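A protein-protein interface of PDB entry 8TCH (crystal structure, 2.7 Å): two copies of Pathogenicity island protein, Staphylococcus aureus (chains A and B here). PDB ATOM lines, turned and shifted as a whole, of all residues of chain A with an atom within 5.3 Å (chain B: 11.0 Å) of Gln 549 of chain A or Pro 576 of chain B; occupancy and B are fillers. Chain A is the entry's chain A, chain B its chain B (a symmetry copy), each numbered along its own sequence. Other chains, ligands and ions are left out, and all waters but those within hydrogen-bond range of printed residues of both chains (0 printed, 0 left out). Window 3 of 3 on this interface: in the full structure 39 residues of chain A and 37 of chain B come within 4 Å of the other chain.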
ATOM      1  N   LYS A 547     -14.843  15.391  16.352  1.00  0.00           N
ATOM      2  CA  LYS A 547     -14.598  15.424  14.918  1.00  0.00           C
ATOM      3  C   LYS A 547     -15.695  14.729  14.124  1.00  0.00           C
ATOM      4  O   LYS A 547     -16.181  13.662  14.512  1.00  0.00           O
ATOM      5  CB  LYS A 547     -13.268  14.762  14.550  1.00  0.00           C
ATOM      6  CG  LYS A 547     -12.919  14.954  13.077  1.00  0.00           C
ATOM      7  CD  LYS A 547     -11.754  14.095  12.666  1.00  0.00           C
ATOM      8  CE  LYS A 547     -12.137  13.016  11.671  1.00  0.00           C
ATOM      9  NZ  LYS A 547     -11.767  13.402  10.280  1.00  0.00           N
ATOM     10  N   HIS A 548     -16.097  15.355  13.019  1.00  0.00           N
ATOM     11  CA  HIS A 548     -16.884  14.649  12.020  1.00  0.00           C
ATOM     12  C   HIS A 548     -16.452  15.083  10.625  1.00  0.00           C
ATOM     13  O   HIS A 548     -16.192  16.267  10.382  1.00  0.00           O
ATOM     14  CB  HIS A 548     -18.387  14.871  12.187  1.00  0.00           C
ATOM     15  CG  HIS A 548     -19.205  14.175  11.144  1.00  0.00           C
ATOM     16  ND1 HIS A 548     -19.261  12.801  11.040  1.00  0.00           N
ATOM     17  CD2 HIS A 548     -19.991  14.660  10.154  1.00  0.00           C
ATOM     18  CE1 HIS A 548     -20.045  12.470  10.029  1.00  0.00           C
ATOM     19  NE2 HIS A 548     -20.506  13.580   9.479  1.00  0.00           N
ATOM     20  N   GLN A 549     -16.368  14.105   9.720  1.00  0.00           N
ATOM     21  CA  GLN A 549     -15.794  14.308   8.394  1.00  0.00           C
ATOM     22  C   GLN A 549     -14.510  15.123   8.475  1.00  0.00           C
ATOM     23  O   GLN A 549     -13.514  14.659   9.040  1.00  0.00           O
ATOM     24  CB  GLN A 549     -16.813  14.949   7.452  1.00  0.00           C
ATOM     25  CG  GLN A 549     -17.957  14.005   7.098  1.00  0.00           C
ATOM     26  CD  GLN A 549     -17.474  12.748   6.388  1.00  0.00           C
ATOM     27  OE1 GLN A 549     -16.952  12.811   5.275  1.00  0.00           O
ATOM     28  NE2 GLN A 549     -17.632  11.601   7.041  1.00  0.00           N
ATOM     29  N   THR A 550     -14.526  16.346   7.951  1.00  0.00           N
ATOM     30  CA  THR A 550     -13.304  17.123   7.828  1.00  0.00           C
ATOM     31  C   THR A 550     -13.202  18.242   8.855  1.00  0.00           C
ATOM     32  O   THR A 550     -12.328  19.106   8.725  1.00  0.00           O
ATOM     33  CB  THR A 550     -13.226  17.744   6.426  1.00  0.00           C
ATOM     34  OG1 THR A 550     -14.378  18.573   6.208  1.00  0.00           O
ATOM     35  CG2 THR A 550     -13.200  16.669   5.350  1.00  0.00           C
ATOM     36  N   VAL A 551     -14.063  18.251   9.869  1.00  0.00           N
ATOM     37  CA  VAL A 551     -14.055  19.332  10.843  1.00  0.00           C
ATOM     38  C   VAL A 551     -13.933  18.824  12.271  1.00  0.00           C
ATOM     39  O   VAL A 551     -14.370  17.715  12.603  1.00  0.00           O
ATOM     40  CB  VAL A 551     -15.317  20.225  10.714  1.00  0.00           C
ATOM     41  CG1 VAL A 551     -15.257  21.394  11.690  1.00  0.00           C
ATOM     42  CG2 VAL A 551     -15.460  20.739   9.287  1.00  0.00           C
ATOM     43  N   ARG B 481     -20.226  27.222   9.370  1.00  0.00           N
ATOM     44  CA  ARG B 481     -19.174  27.099   8.366  1.00  0.00           C
ATOM     45  C   ARG B 481     -19.729  27.027   6.951  1.00  0.00           C
ATOM     46  O   ARG B 481     -18.990  27.305   5.999  1.00  0.00           O
ATOM     47  CB  ARG B 481     -18.293  25.883   8.657  1.00  0.00           C
ATOM     48  CG  ARG B 481     -17.565  25.968   9.994  1.00  0.00           C
ATOM     49  CD  ARG B 481     -17.357  24.597  10.601  1.00  0.00           C
ATOM     50  NE  ARG B 481     -16.441  24.612  11.738  1.00  0.00           N
ATOM     51  CZ  ARG B 481     -15.115  24.593  11.629  1.00  0.00           C
ATOM     52  NH1 ARG B 481     -14.544  24.570  10.431  1.00  0.00           N
ATOM     53  NH2 ARG B 481     -14.360  24.593  12.719  1.00  0.00           N
ATOM     54  N   ASN B 482     -21.016  26.680   6.788  1.00  0.00           N
ATOM     55  CA  ASN B 482     -21.638  26.784   5.474  1.00  0.00           C
ATOM     56  C   ASN B 482     -21.658  28.216   4.976  1.00  0.00           C
ATOM     57  O   ASN B 482     -22.058  28.453   3.827  1.00  0.00           O
ATOM     58  CB  ASN B 482     -23.076  26.240   5.525  1.00  0.00           C
ATOM     59  CG  ASN B 482     -23.136  24.725   5.602  1.00  0.00           C
ATOM     60  OD1 ASN B 482     -22.140  24.036   5.377  1.00  0.00           O
ATOM     61  ND2 ASN B 482     -24.314  24.198   5.916  1.00  0.00           N
ATOM     62  N   GLY B 488      -9.678  25.267   1.774  1.00  0.00           N
ATOM     63  CA  GLY B 488     -10.347  24.026   2.088  1.00  0.00           C
ATOM     64  C   GLY B 488     -11.850  24.130   2.205  1.00  0.00           C
ATOM     65  O   GLY B 488     -12.505  23.116   2.483  1.00  0.00           O
ATOM     66  N   ASP B 569     -10.749  25.314  15.961  1.00  0.00           N
ATOM     67  CA  ASP B 569      -9.951  24.780  14.856  1.00  0.00           C
ATOM     68  C   ASP B 569     -10.826  24.901  13.607  1.00  0.00           C
ATOM     69  O   ASP B 569     -11.583  23.988  13.272  1.00  0.00           O
ATOM     70  CB  ASP B 569      -9.538  23.340  15.124  1.00  0.00           C
ATOM     71  CG  ASP B 569      -8.434  22.871  14.203  1.00  0.00           C
ATOM     72  OD1 ASP B 569      -8.113  23.596  13.235  1.00  0.00           O
ATOM     73  OD2 ASP B 569      -7.883  21.778  14.447  1.00  0.00           O
ATOM     74  N   SER B 571     -10.119  24.734  10.533  1.00  0.00           N
ATOM     75  CA  SER B 571      -9.699  24.083   9.304  1.00  0.00           C
ATOM     76  C   SER B 571     -10.837  23.204   8.795  1.00  0.00           C
ATOM     77  O   SER B 571     -11.489  22.498   9.568  1.00  0.00           O
ATOM     78  CB  SER B 571      -8.449  23.241   9.535  1.00  0.00           C
ATOM     79  OG  SER B 571      -8.048  22.619   8.328  1.00  0.00           O
ATOM     80  N   ASN B 572     -11.068  23.243   7.485  1.00  0.00           N
ATOM     81  CA  ASN B 572     -12.041  22.375   6.840  1.00  0.00           C
ATOM     82  C   ASN B 572     -11.380  21.192   6.152  1.00  0.00           C
ATOM     83  O   ASN B 572     -12.049  20.451   5.425  1.00  0.00           O
ATOM     84  CB  ASN B 572     -12.873  23.165   5.826  1.00  0.00           C
ATOM     85  CG  ASN B 572     -14.180  22.472   5.474  1.00  0.00           C
ATOM     86  OD1 ASN B 572     -14.844  21.896   6.336  1.00  0.00           O
ATOM     87  ND2 ASN B 572     -14.547  22.515   4.201  1.00  0.00           N
ATOM     88  N   SER B 573     -10.077  21.013   6.353  1.00  0.00           N
ATOM     89  CA  SER B 573      -9.312  19.944   5.724  1.00  0.00           C
ATOM     90  C   SER B 573      -8.900  18.951   6.801  1.00  0.00           C
ATOM     91  O   SER B 573      -8.047  19.250   7.643  1.00  0.00           O
ATOM     92  CB  SER B 573      -8.095  20.499   4.990  1.00  0.00           C
ATOM     93  OG  SER B 573      -7.454  19.474   4.255  1.00  0.00           O
ATOM     94  N   TYR B 574      -9.515  17.774   6.777  1.00  0.00           N
ATOM     95  CA  TYR B 574      -9.194  16.700   7.706  1.00  0.00           C
ATOM     96  C   TYR B 574      -9.738  15.438   7.061  1.00  0.00           C
ATOM     97  O   TYR B 574     -10.930  15.375   6.749  1.00  0.00           O
ATOM     98  CB  TYR B 574      -9.826  16.901   9.078  1.00  0.00           C
ATOM     99  CG  TYR B 574      -9.023  17.719  10.070  1.00  0.00           C
ATOM    100  CD1 TYR B 574      -7.875  17.210  10.671  1.00  0.00           C
ATOM    101  CD2 TYR B 574      -9.447  18.987  10.445  1.00  0.00           C
ATOM    102  CE1 TYR B 574      -7.158  17.961  11.595  1.00  0.00           C
ATOM    103  CE2 TYR B 574      -8.740  19.739  11.362  1.00  0.00           C
ATOM    104  CZ  TYR B 574      -7.597  19.225  11.936  1.00  0.00           C
ATOM    105  OH  TYR B 574      -6.898  19.982  12.851  1.00  0.00           O
ATOM    106  N   ASN B 575      -8.892  14.447   6.851  1.00  0.00           N
ATOM    107  CA  ASN B 575      -9.341  13.259   6.151  1.00  0.00           C
ATOM    108  C   ASN B 575     -10.611  12.717   6.809  1.00  0.00           C
ATOM    109  O   ASN B 575     -10.667  12.613   8.042  1.00  0.00           O
ATOM    110  CB  ASN B 575      -8.254  12.193   6.149  1.00  0.00           C
ATOM    111  CG  ASN B 575      -8.543  11.094   5.162  1.00  0.00           C
ATOM    112  OD1 ASN B 575      -9.241  11.302   4.170  1.00  0.00           O
ATOM    113  ND2 ASN B 575      -8.013   9.911   5.427  1.00  0.00           N
ATOM    114  N   PRO B 576     -11.644  12.393   6.032  1.00  0.00           N
ATOM    115  CA  PRO B 576     -12.866  11.844   6.639  1.00  0.00           C
ATOM    116  C   PRO B 576     -12.637  10.576   7.448  1.00  0.00           C
ATOM    117  O   PRO B 576     -13.401  10.309   8.384  1.00  0.00           O
ATOM    118  CB  PRO B 576     -13.766  11.582   5.420  1.00  0.00           C
ATOM    119  CG  PRO B 576     -13.272  12.532   4.373  1.00  0.00           C
ATOM    120  CD  PRO B 576     -11.798  12.638   4.587  1.00  0.00           C
ATOM    121  N   ASN B 577     -11.599   9.793   7.133  1.00  0.00           N
ATOM    122  CA  ASN B 577     -11.469   8.433   7.658  1.00  0.00           C
ATOM    123  C   ASN B 577     -11.175   8.383   9.154  1.00  0.00           C
ATOM    124  O   ASN B 577     -11.136   7.273   9.711  1.00  0.00           O
ATOM    125  CB  ASN B 577     -10.363   7.695   6.899  1.00  0.00           C
ATOM    126  CG  ASN B 577     -10.777   7.298   5.492  1.00  0.00           C
ATOM    127  OD1 ASN B 577     -11.963   7.266   5.167  1.00  0.00           O
ATOM    128  ND2 ASN B 577      -9.795   6.982   4.652  1.00  0.00           N
ATOM    129  N   SER B 578     -10.988   9.509   9.821  1.00  0.00           N
ATOM    130  CA  SER B 578     -10.545   9.505  11.208  1.00  0.00           C
ATOM    131  C   SER B 578     -11.693   9.650  12.204  1.00  0.00           C
ATOM    132  O   SER B 578     -11.517   9.412  13.398  1.00  0.00           O
ATOM    133  CB  SER B 578      -9.524  10.611  11.425  1.00  0.00           C
ATOM    134  OG  SER B 578      -8.450  10.497  10.514  1.00  0.00           O
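O of Asn 575 of chain B lies within hydrogen-bond range of NZ of Lys 547 of chain A (2.6 Å). The side-chain hydroxyl (OG1) of Thr 550 of chain A sits at hydrogen-bond distance from the backbone carbonyl oxygen (O) of Asn 572 of chain B (3.1 Å).
Among the printed residues, pairs that only touch across the chains: Lys 547 of chain A with Pro 576 of chain B (3.98 Å), Lys 547 of chain A with Ser 578 of chain B (3.4 Å), Gln 549 of chain A with Tyr 574 of chain B (3.5 Å), Gln 549 of chain A with Asn 575 of chain B (3.6 Å), Gln 549 of chain A with Pro 576 of chain B (3.4 Å), Thr 550 of chain A with Ser 571 of chain B (3.6 Å), Thr 550 of chain A with Ser 573 of chain B (3.8 Å), Thr 550 of chain A with Tyr 574 of chain B (3.0 Å), Val 551 of chain A with Arg 481 of chain B (3.2 Å) and Val 551 of chain A with Asn 572 of chain B (3.2 Å).
No position is printed for both chains. Of the 12 pairs that touch across the chains among the printed residues, none has its exchanged pair printed and touching as well.
Hydrophobic or aromatic side chains of chain A that line the printed part of chain B: Val 551. Of the 12 printed residues of chain B, 8 touch a printed residue of chain A. Hydrophobic or aromatic side chains of chain B within 4 Å of the printed part of chain A: Tyr 574 and Pro 576. Among the printed residues, no Asp or Glu carboxylate lies within 4 Å of a Lys or Arg side-chain nitrogen of the other chain.
NZ of Lys 547 of chain A sits at hydrogen-bond distance from O of Gln 549 of chain A (2.5 Å). NH2 of Arg 481 of chain B is in hydrogen-bond range of O of Asp 569 of chain B, 2.9 Å away. ND2 of Asn 572 of chain B sits at hydrogen-bond distance from O of Gly 488 of chain B (2.7 Å). The side-chain carboxylate of Asp 569 of chain B is in hydrogen-bond range of the side-chain hydroxyl of Tyr 574 of chain B (2.6 Å). N of Ser 573 of chain B is in hydrogen-bond range of OG of Ser 571 of chain B.
Of chain B, only Tyr 574 (3.5 Å), Asn 575 (3.6 Å) and Pro 576 (3.4 Å) come within 4 Å of Gln 549 of chain A. Of chain A, only Lys 547 (3.98 Å) and Gln 549 (3.4 Å) come within 4 Å of Pro 576 of chain B. Lys 547 of chain A touches just these residues of chain B: Asn 575, Pro 576 and Ser 578. His 548 of chain A touches none of the printed residues of chain B. Of chain B, only Ser 571 (3.6 Å), Asn 572 (3.1 Å), Ser 573 (3.8 Å) and Tyr 574 (3.0 Å) come within 4 Å of Thr 550 of chain A. Printed residues of chain A within 4 Å of Tyr 574 of chain B: Gln 549 (3.5 Å) and Thr 550 (3.0 Å). Of the printed residues of chain A, Asn 575 of chain B touches Lys 547 and Gln 549. Of the printed residues of chain A, Arg 481 of chain B touches Val 551 (3.2 Å). The nearest residue of chain B that does not touch Gln 549 of chain A is Asn 577 of chain B (5.6 Å). The nearest printed residue of chain A that does not touch Ser 578 of chain B is Gln 549 of chain A (5.8 Å).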
